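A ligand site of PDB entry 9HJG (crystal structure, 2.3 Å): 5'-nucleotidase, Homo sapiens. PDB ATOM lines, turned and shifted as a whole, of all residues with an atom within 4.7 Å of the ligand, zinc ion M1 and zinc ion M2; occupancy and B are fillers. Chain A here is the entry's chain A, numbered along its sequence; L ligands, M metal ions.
The side-chain amide oxygen (OD1) of Asn 91 is bound to zinc ion M2.
An oxygen (O4) of the ligand is bound to zinc ion M2.
Zinc ion M2 is bound by NE2 of His 194, at 2.3 Å.
Zinc ion M2 is bound by OD2 of Asp 59 (2.3 Å).
ND1 of His 217 is bound to zinc ion M2, 2.3 Å away.
Zinc ion M2 has five donor atoms within binding distance.
Slightly farther from zinc ion M2 lies O2 of the ligand (2.8 Å).
Zinc ion M1 is bound by OD2 of Asp 10 (1.9 Å), NE2 of His 12 (2.3 Å), O2 of the ligand (2.3 Å), OD2 of Asp 59 (2.4 Å) and O3 of the ligand (2.5 Å).
Zinc ion M1 has five donor atoms within binding distance.
Four residues have an atom within 4 Å of zinc ion M2: Asp 59, Asn 91, His 194 and His 217.
The side-chain carboxylate (OD2) of Asp 95 is in hydrogen-bond range of a ring nitrogen (ND1) of His 92, at 2.6 Å.
The side-chain carboxylate (OD1) of Asp 59 lies within hydrogen-bond range of the backbone NH (N) of His 92 (3.1 Å).
NH2 of Arg 369 lies within hydrogen-bond range of NE2 of His 92.
The backbone carbonyl oxygen (O) of Asn 91 sits at hydrogen-bond distance from the side-chain hydroxyl (OG) of Ser 159 (3.0 Å).
The side-chain hydroxyl of Ser 159 is in hydrogen-bond range of the side-chain carboxylate of Asp 95 (2.6 Å).
The backbone carbonyl oxygen (O) of Asn 473 lies close to the side-chain amide oxygen (OD1) of Asn 477.
OD1 of Asp 10 is in hydrogen-bond range of N of His 217 (2.9 Å).
NH1 of Arg 369 is in hydrogen-bond range of O of Gly 366, at 3.4 Å.
OD1 of Asp 95 touches C15 of the ligand (3.7 Å).
O of Leu 158 touches C9 of the ligand, 3.6 Å away.
Asn 160 touches the ligand.
Gly 366 touches the ligand.
Phe 391 touches the ligand (O to C7, 3.1 Å).
Pro 472 touches the ligand.
ND2 of Asn 473 touches C4 of the ligand (3.6 Å).
CB of Phe 474 touches C16 of the ligand, at 3.3 Å.
Of the 23 residues printed, 16 come within 4 Å of the ligand.
The nearest printed residue that does not touch zinc ion M1 is Asn 219 (4.1 Å).
A ring nitrogen (NE2) of His 92 sits close to an oxygen (O3) of the ligand, at 2.8 Å.
An oxygen (O5) of the ligand lies within salt-bridge range of the guanidinium group (NH1) of Arg 369 (2.7 Å).
The guanidinium group (NH2) of Arg 328 lies within salt-bridge range of an oxygen (O5) of the ligand.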
ATOM      1  N   ASP A  10       9.657  -1.235 -12.213  1.00  0.00           N
ATOM      2  CA  ASP A  10      11.014  -1.068 -12.715  1.00  0.00           C
ATOM      3  C   ASP A  10      11.785  -2.385 -12.663  1.00  0.00           C
ATOM      4  O   ASP A  10      12.906  -2.469 -12.151  1.00  0.00           O
ATOM      5  CB  ASP A  10      11.744   0.025 -11.928  1.00  0.00           C
ATOM      6  CG  ASP A  10      11.022   1.349 -11.994  1.00  0.00           C
ATOM      7  OD1 ASP A  10       9.992   1.487 -11.294  1.00  0.00           O
ATOM      8  OD2 ASP A  10      11.480   2.228 -12.738  1.00  0.00           O
ATOM      9  N   HIS A  12      12.779  -4.119 -15.368  1.00  0.00           N
ATOM     10  CA  HIS A  12      13.847  -3.865 -16.346  1.00  0.00           C
ATOM     11  C   HIS A  12      14.570  -5.140 -16.750  1.00  0.00           C
ATOM     12  O   HIS A  12      15.785  -5.286 -16.577  1.00  0.00           O
ATOM     13  CB  HIS A  12      14.834  -2.823 -15.797  1.00  0.00           C
ATOM     14  CG  HIS A  12      14.290  -1.424 -15.761  1.00  0.00           C
ATOM     15  ND1 HIS A  12      13.993  -0.717 -16.913  1.00  0.00           N
ATOM     16  CD2 HIS A  12      13.966  -0.615 -14.730  1.00  0.00           C
ATOM     17  CE1 HIS A  12      13.530   0.479 -16.583  1.00  0.00           C
ATOM     18  NE2 HIS A  12      13.510   0.568 -15.268  1.00  0.00           N
ATOM     19  N   ASP A  59       7.877   0.139 -16.463  1.00  0.00           N
ATOM     20  CA  ASP A  59       9.299  -0.092 -16.692  1.00  0.00           C
ATOM     21  C   ASP A  59       9.661  -1.566 -16.568  1.00  0.00           C
ATOM     22  O   ASP A  59      10.589  -1.952 -15.854  1.00  0.00           O
ATOM     23  CB  ASP A  59      10.143   0.775 -15.758  1.00  0.00           C
ATOM     24  CG  ASP A  59      10.374   2.192 -16.298  1.00  0.00           C
ATOM     25  OD1 ASP A  59       9.762   2.554 -17.319  1.00  0.00           O
ATOM     26  OD2 ASP A  59      11.212   2.929 -15.726  1.00  0.00           O
ATOM     27  N   ASN A  91       7.695   5.052 -18.820  1.00  0.00           N
ATOM     28  CA  ASN A  91       8.385   5.794 -19.857  1.00  0.00           C
ATOM     29  C   ASN A  91       9.229   4.871 -20.743  1.00  0.00           C
ATOM     30  O   ASN A  91       9.307   5.090 -21.961  1.00  0.00           O
ATOM     31  CB  ASN A  91       9.261   6.897 -19.242  1.00  0.00           C
ATOM     32  CG  ASN A  91      10.227   6.361 -18.219  1.00  0.00           C
ATOM     33  OD1 ASN A  91       9.839   6.016 -17.102  1.00  0.00           O
ATOM     34  ND2 ASN A  91      11.508   6.304 -18.591  1.00  0.00           N
ATOM     35  N   HIS A  92       9.825   3.812 -20.165  1.00  0.00           N
ATOM     36  CA  HIS A  92      10.678   2.931 -20.959  1.00  0.00           C
ATOM     37  C   HIS A  92       9.890   1.982 -21.859  1.00  0.00           C
ATOM     38  O   HIS A  92      10.477   1.409 -22.781  1.00  0.00           O
ATOM     39  CB  HIS A  92      11.618   2.113 -20.069  1.00  0.00           C
ATOM     40  CG  HIS A  92      12.791   2.897 -19.557  1.00  0.00           C
ATOM     41  ND1 HIS A  92      13.815   3.309 -20.371  1.00  0.00           N
ATOM     42  CD2 HIS A  92      13.086   3.350 -18.314  1.00  0.00           C
ATOM     43  CE1 HIS A  92      14.704   3.984 -19.662  1.00  0.00           C
ATOM     44  NE2 HIS A  92      14.286   4.021 -18.411  1.00  0.00           N
ATOM     45  N   ASP A  95      10.679   3.142 -25.334  1.00  0.00           N
ATOM     46  CA  ASP A  95      12.041   3.287 -25.835  1.00  0.00           C
ATOM     47  C   ASP A  95      12.156   2.845 -27.287  1.00  0.00           C
ATOM     48  O   ASP A  95      12.970   3.381 -28.038  1.00  0.00           O
ATOM     49  CB  ASP A  95      12.998   2.473 -24.969  1.00  0.00           C
ATOM     50  CG  ASP A  95      13.288   3.144 -23.651  1.00  0.00           C
ATOM     51  OD1 ASP A  95      12.771   4.264 -23.430  1.00  0.00           O
ATOM     52  OD2 ASP A  95      14.021   2.540 -22.837  1.00  0.00           O
ATOM     53  N   LEU A 158      12.282  11.496 -21.944  1.00  0.00           N
ATOM     54  CA  LEU A 158      13.009  10.320 -21.480  1.00  0.00           C
ATOM     55  C   LEU A 158      12.993   9.150 -22.464  1.00  0.00           C
ATOM     56  O   LEU A 158      13.809   8.234 -22.309  1.00  0.00           O
ATOM     57  CB  LEU A 158      12.429   9.839 -20.137  1.00  0.00           C
ATOM     58  CG  LEU A 158      12.159  10.874 -19.045  1.00  0.00           C
ATOM     59  CD1 LEU A 158      11.381  10.242 -17.887  1.00  0.00           C
ATOM     60  CD2 LEU A 158      13.443  11.470 -18.507  1.00  0.00           C
ATOM     61  N   SER A 159      12.086   9.138 -23.441  1.00  0.00           N
ATOM     62  CA  SER A 159      11.939   7.992 -24.328  1.00  0.00           C
ATOM     63  C   SER A 159      11.624   8.406 -25.765  1.00  0.00           C
ATOM     64  O   SER A 159      12.046   9.477 -26.204  1.00  0.00           O
ATOM     65  CB  SER A 159      10.877   7.038 -23.791  1.00  0.00           C
ATOM     66  OG  SER A 159      10.951   5.779 -24.428  1.00  0.00           O
ATOM     67  N   ASN A 160      10.876   7.573 -26.499  1.00  0.00           N
ATOM     68  CA  ASN A 160      10.582   7.827 -27.918  1.00  0.00           C
ATOM     69  C   ASN A 160       9.103   7.607 -28.221  1.00  0.00           C
ATOM     70  O   ASN A 160       8.741   6.859 -29.124  1.00  0.00           O
ATOM     71  CB  ASN A 160      11.466   6.951 -28.804  1.00  0.00           C
ATOM     72  CG  ASN A 160      11.409   7.351 -30.283  1.00  0.00           C
ATOM     73  OD1 ASN A 160      10.953   8.441 -30.646  1.00  0.00           O
ATOM     74  ND2 ASN A 160      11.914   6.468 -31.144  1.00  0.00           N
ATOM     75  N   HIS A 194       3.406   5.317 -13.086  1.00  0.00           N
ATOM     76  CA  HIS A 194       4.856   5.391 -13.205  1.00  0.00           C
ATOM     77  C   HIS A 194       5.290   6.843 -13.406  1.00  0.00           C
ATOM     78  O   HIS A 194       5.607   7.268 -14.511  1.00  0.00           O
ATOM     79  CB  HIS A 194       5.317   4.517 -14.368  1.00  0.00           C
ATOM     80  CG  HIS A 194       6.791   4.258 -14.375  1.00  0.00           C
ATOM     81  ND1 HIS A 194       7.362   3.218 -13.684  1.00  0.00           N
ATOM     82  CD2 HIS A 194       7.805   4.925 -14.976  1.00  0.00           C
ATOM     83  CE1 HIS A 194       8.664   3.244 -13.850  1.00  0.00           C
ATOM     84  NE2 HIS A 194       8.969   4.273 -14.622  1.00  0.00           N
ATOM     85  N   HIS A 217       9.289   4.238 -10.923  1.00  0.00           N
ATOM     86  CA  HIS A 217      10.117   5.230 -11.625  1.00  0.00           C
ATOM     87  C   HIS A 217      11.270   5.776 -10.781  1.00  0.00           C
ATOM     88  O   HIS A 217      12.376   5.980 -11.310  1.00  0.00           O
ATOM     89  CB  HIS A 217       9.255   6.400 -12.111  1.00  0.00           C
ATOM     90  CG  HIS A 217       9.969   7.359 -13.003  1.00  0.00           C
ATOM     91  ND1 HIS A 217      10.491   7.002 -14.227  1.00  0.00           N
ATOM     92  CD2 HIS A 217      10.243   8.682 -12.855  1.00  0.00           C
ATOM     93  CE1 HIS A 217      11.061   8.047 -14.795  1.00  0.00           C
ATOM     94  NE2 HIS A 217      10.925   9.088 -13.984  1.00  0.00           N
ATOM     95  N   ASN A 219      12.553   4.172  -8.092  1.00  0.00           N
ATOM     96  CA  ASN A 219      13.187   3.043  -7.407  1.00  0.00           C
ATOM     97  C   ASN A 219      13.128   3.246  -5.882  1.00  0.00           C
ATOM     98  O   ASN A 219      14.073   2.920  -5.155  1.00  0.00           O
ATOM     99  CB  ASN A 219      14.616   2.776  -7.855  1.00  0.00           C
ATOM    100  CG  ASN A 219      14.726   2.554  -9.334  1.00  0.00           C
ATOM    101  OD1 ASN A 219      13.730   2.553 -10.047  1.00  0.00           O
ATOM    102  ND2 ASN A 219      15.936   2.250  -9.792  1.00  0.00           N
ATOM    103  N   ARG A 328      25.514  10.010 -12.263  1.00  0.00           N
ATOM    104  CA  ARG A 328      24.570  11.105 -12.428  1.00  0.00           C
ATOM    105  C   ARG A 328      24.865  12.289 -11.512  1.00  0.00           C
ATOM    106  O   ARG A 328      24.089  13.247 -11.484  1.00  0.00           O
ATOM    107  CB  ARG A 328      23.159  10.596 -12.176  1.00  0.00           C
ATOM    108  CG  ARG A 328      22.779   9.455 -13.096  1.00  0.00           C
ATOM    109  CD  ARG A 328      21.280   9.218 -13.140  1.00  0.00           C
ATOM    110  NE  ARG A 328      20.973   7.967 -13.827  1.00  0.00           N
ATOM    111  CZ  ARG A 328      19.747   7.522 -14.035  1.00  0.00           C
ATOM    112  NH1 ARG A 328      18.683   8.207 -13.654  1.00  0.00           N
ATOM    113  NH2 ARG A 328      19.576   6.344 -14.645  1.00  0.00           N
ATOM    114  N   ASN A 364      25.233  10.970 -21.835  1.00  0.00           N
ATOM    115  CA  ASN A 364      24.253  11.221 -20.785  1.00  0.00           C
ATOM    116  C   ASN A 364      24.318  10.117 -19.733  1.00  0.00           C
ATOM    117  O   ASN A 364      24.135   8.937 -20.058  1.00  0.00           O
ATOM    118  CB  ASN A 364      22.846  11.341 -21.370  1.00  0.00           C
ATOM    119  CG  ASN A 364      22.475  10.148 -22.239  1.00  0.00           C
ATOM    120  OD1 ASN A 364      23.236   9.731 -23.104  1.00  0.00           O
ATOM    121  ND2 ASN A 364      21.294   9.587 -21.997  1.00  0.00           N
ATOM    122  N   GLY A 366      22.268   9.109 -17.663  1.00  0.00           N
ATOM    123  CA  GLY A 366      21.081   8.278 -17.628  1.00  0.00           C
ATOM    124  C   GLY A 366      21.064   7.181 -18.651  1.00  0.00           C
ATOM    125  O   GLY A 366      20.166   6.318 -18.600  1.00  0.00           O
ATOM    126  N   ARG A 369      23.239   2.135 -17.569  1.00  0.00           N
ATOM    127  CA  ARG A 369      22.148   1.492 -16.859  1.00  0.00           C
ATOM    128  C   ARG A 369      22.578   0.447 -15.839  1.00  0.00           C
ATOM    129  O   ARG A 369      21.714  -0.136 -15.189  1.00  0.00           O
ATOM    130  CB  ARG A 369      21.175   0.863 -17.869  1.00  0.00           C
ATOM    131  CG  ARG A 369      20.690   1.815 -18.942  1.00  0.00           C
ATOM    132  CD  ARG A 369      19.847   2.916 -18.312  1.00  0.00           C
ATOM    133  NE  ARG A 369      18.635   2.383 -17.699  1.00  0.00           N
ATOM    134  CZ  ARG A 369      17.622   3.119 -17.297  1.00  0.00           C
ATOM    135  NH1 ARG A 369      17.620   4.435 -17.438  1.00  0.00           N
ATOM    136  NH2 ARG A 369      16.566   2.518 -16.745  1.00  0.00           N
ATOM    137  N   PHE A 391      20.204  -0.271 -24.777  1.00  0.00           N
ATOM    138  CA  PHE A 391      19.267   0.358 -25.690  1.00  0.00           C
ATOM    139  C   PHE A 391      19.497   0.000 -27.138  1.00  0.00           C
ATOM    140  O   PHE A 391      18.588   0.144 -27.960  1.00  0.00           O
ATOM    141  CB  PHE A 391      19.344   1.880 -25.564  1.00  0.00           C
ATOM    142  CG  PHE A 391      19.043   2.411 -24.190  1.00  0.00           C
ATOM    143  CD1 PHE A 391      17.750   2.358 -23.690  1.00  0.00           C
ATOM    144  CD2 PHE A 391      20.041   2.935 -23.384  1.00  0.00           C
ATOM    145  CE1 PHE A 391      17.459   2.843 -22.427  1.00  0.00           C
ATOM    146  CE2 PHE A 391      19.763   3.410 -22.126  1.00  0.00           C
ATOM    147  CZ  PHE A 391      18.466   3.369 -21.644  1.00  0.00           C
ATOM    148  N   GLY A 393      21.626   1.584 -29.151  1.00  0.00           N
ATOM    149  CA  GLY A 393      21.831   2.814 -29.888  1.00  0.00           C
ATOM    150  C   GLY A 393      23.209   2.849 -30.511  1.00  0.00           C
ATOM    151  O   GLY A 393      24.012   1.935 -30.368  1.00  0.00           O
ATOM    152  N   SER A 419      19.021  13.486  -9.215  1.00  0.00           N
ATOM    153  CA  SER A 419      19.382  12.229  -9.878  1.00  0.00           C
ATOM    154  C   SER A 419      18.883  12.177 -11.309  1.00  0.00           C
ATOM    155  O   SER A 419      18.549  11.108 -11.823  1.00  0.00           O
ATOM    156  CB  SER A 419      18.852  11.033  -9.091  1.00  0.00           C
ATOM    157  OG  SER A 419      19.390   9.829  -9.608  1.00  0.00           O
ATOM    158  N   PRO A 472      25.885   9.648 -28.124  1.00  0.00           N
ATOM    159  CA  PRO A 472      24.854   8.682 -28.511  1.00  0.00           C
ATOM    160  C   PRO A 472      23.847   9.333 -29.450  1.00  0.00           C
ATOM    161  O   PRO A 472      23.612  10.534 -29.411  1.00  0.00           O
ATOM    162  CB  PRO A 472      24.191   8.285 -27.181  1.00  0.00           C
ATOM    163  CG  PRO A 472      25.141   8.734 -26.121  1.00  0.00           C
ATOM    164  CD  PRO A 472      25.862   9.928 -26.674  1.00  0.00           C
ATOM    165  N   ASN A 473      23.262   8.501 -30.316  1.00  0.00           N
ATOM    166  CA  ASN A 473      22.207   8.999 -31.185  1.00  0.00           C
ATOM    167  C   ASN A 473      21.051   9.596 -30.395  1.00  0.00           C
ATOM    168  O   ASN A 473      20.353  10.484 -30.884  1.00  0.00           O
ATOM    169  CB  ASN A 473      21.686   7.865 -32.056  1.00  0.00           C
ATOM    170  CG  ASN A 473      21.078   6.742 -31.243  1.00  0.00           C
ATOM    171  OD1 ASN A 473      21.538   6.445 -30.125  1.00  0.00           O
ATOM    172  ND2 ASN A 473      20.040   6.116 -31.779  1.00  0.00           N
ATOM    173  N   PHE A 474      20.842   9.123 -29.158  1.00  0.00           N
ATOM    174  CA  PHE A 474      19.771   9.650 -28.328  1.00  0.00           C
ATOM    175  C   PHE A 474      19.977  11.140 -28.033  1.00  0.00           C
ATOM    176  O   PHE A 474      19.002  11.904 -27.987  1.00  0.00           O
ATOM    177  CB  PHE A 474      19.686   8.878 -27.017  1.00  0.00           C
ATOM    178  CG  PHE A 474      18.623   9.373 -26.079  1.00  0.00           C
ATOM    179  CD1 PHE A 474      17.291   9.064 -26.283  1.00  0.00           C
ATOM    180  CD2 PHE A 474      18.969  10.145 -24.972  1.00  0.00           C
ATOM    181  CE1 PHE A 474      16.323   9.520 -25.423  1.00  0.00           C
ATOM    182  CE2 PHE A 474      18.001  10.602 -24.113  1.00  0.00           C
ATOM    183  CZ  PHE A 474      16.676  10.294 -24.340  1.00  0.00           C
ATOM    184  N   ASN A 477      19.504  13.575 -31.190  1.00  0.00           N
ATOM    185  CA  ASN A 477      18.118  13.844 -31.514  1.00  0.00           C
ATOM    186  C   ASN A 477      17.389  14.639 -30.431  1.00  0.00           C
ATOM    187  O   ASN A 477      16.151  14.631 -30.398  1.00  0.00           O
ATOM    188  CB  ASN A 477      17.385  12.531 -31.773  1.00  0.00           C
ATOM    189  CG  ASN A 477      17.989  11.718 -32.907  1.00  0.00           C
ATOM    190  OD1 ASN A 477      18.437  10.594 -32.708  1.00  0.00           O
ATOM    191  ND2 ASN A 477      18.086  12.330 -34.086  1.00  0.00           N
HETATM  192  N1  LIG L   1      19.493   6.355 -24.596  1.00  0.00           N
HETATM  193  C1  LIG L   1      18.180   6.045 -24.618  1.00  0.00           C
HETATM  194  C2  LIG L   1      17.539   5.334 -25.618  1.00  0.00           C
HETATM  195  C3  LIG L   1      18.320   4.940 -26.734  1.00  0.00           C
HETATM  196  C4  LIG L   1      17.812   5.150 -29.124  1.00  0.00           C
HETATM  197  C5  LIG L   1      16.840   7.336 -29.912  1.00  0.00           C
HETATM  198  C6  LIG L   1      14.746   7.128 -28.126  1.00  0.00           C
HETATM  199  C7  LIG L   1      17.325   3.002 -28.028  1.00  0.00           C
HETATM  200  C8  LIG L   1      17.381   7.309 -22.574  1.00  0.00           C
HETATM  201  C9  LIG L   1      16.887   6.730 -21.243  1.00  0.00           C
HETATM  202  C10 LIG L   1      16.708   7.806 -20.170  1.00  0.00           C
HETATM  203  C11 LIG L   1      15.505   8.271 -17.958  1.00  0.00           C
HETATM  204  C12 LIG L   1      15.892   8.334 -29.843  1.00  0.00           C
HETATM  205  C13 LIG L   1      14.840   8.231 -28.945  1.00  0.00           C
HETATM  206  C14 LIG L   1      15.704   6.132 -28.196  1.00  0.00           C
HETATM  207  C15 LIG L   1      16.052   5.867 -24.179  1.00  0.00           C
HETATM  208  C16 LIG L   1      20.103   5.913 -25.679  1.00  0.00           C
HETATM  209  C17 LIG L   1      16.175   7.253 -18.854  1.00  0.00           C
HETATM  210  C18 LIG L   1      14.980   6.049 -14.607  1.00  0.00           C
HETATM  211  C19 LIG L   1      16.761   6.218 -29.085  1.00  0.00           C
HETATM  212  N2  LIG L   1      19.634   5.245 -26.720  1.00  0.00           N
HETATM  213  N3  LIG L   1      16.167   5.229 -25.320  1.00  0.00           N
HETATM  214  N4  LIG L   1      17.226   6.382 -23.704  1.00  0.00           N
HETATM  215  N5  LIG L   1      17.838   4.363 -27.881  1.00  0.00           N
HETATM  216  O1  LIG L   1      15.043   7.595 -16.756  1.00  0.00           O
HETATM  217  O2  LIG L   1      12.904   4.587 -13.782  1.00  0.00           O
HETATM  218  O3  LIG L   1      14.340   3.630 -15.642  1.00  0.00           O
HETATM  219  O4  LIG L   1      12.816   5.592 -16.099  1.00  0.00           O
HETATM  220  O5  LIG L   1      17.280   6.662 -15.922  1.00  0.00           O
HETATM  221  O6  LIG L   1      15.980   8.547 -14.705  1.00  0.00           O
HETATM  222  P1  LIG L   1      15.982   7.270 -15.483  1.00  0.00           P
HETATM  223  P2  LIG L   1      13.670   4.881 -15.075  1.00  0.00           P
HETATM  224 CL1  LIG L   1      21.808   6.306 -25.769  1.00  0.00          CL
HETATM  225 ZN    ZN M   1      12.793   2.346 -14.078  1.00  0.00          ZN
HETATM  226 ZN    ZN M   2      10.813   5.167 -15.557  1.00  0.00          ZN
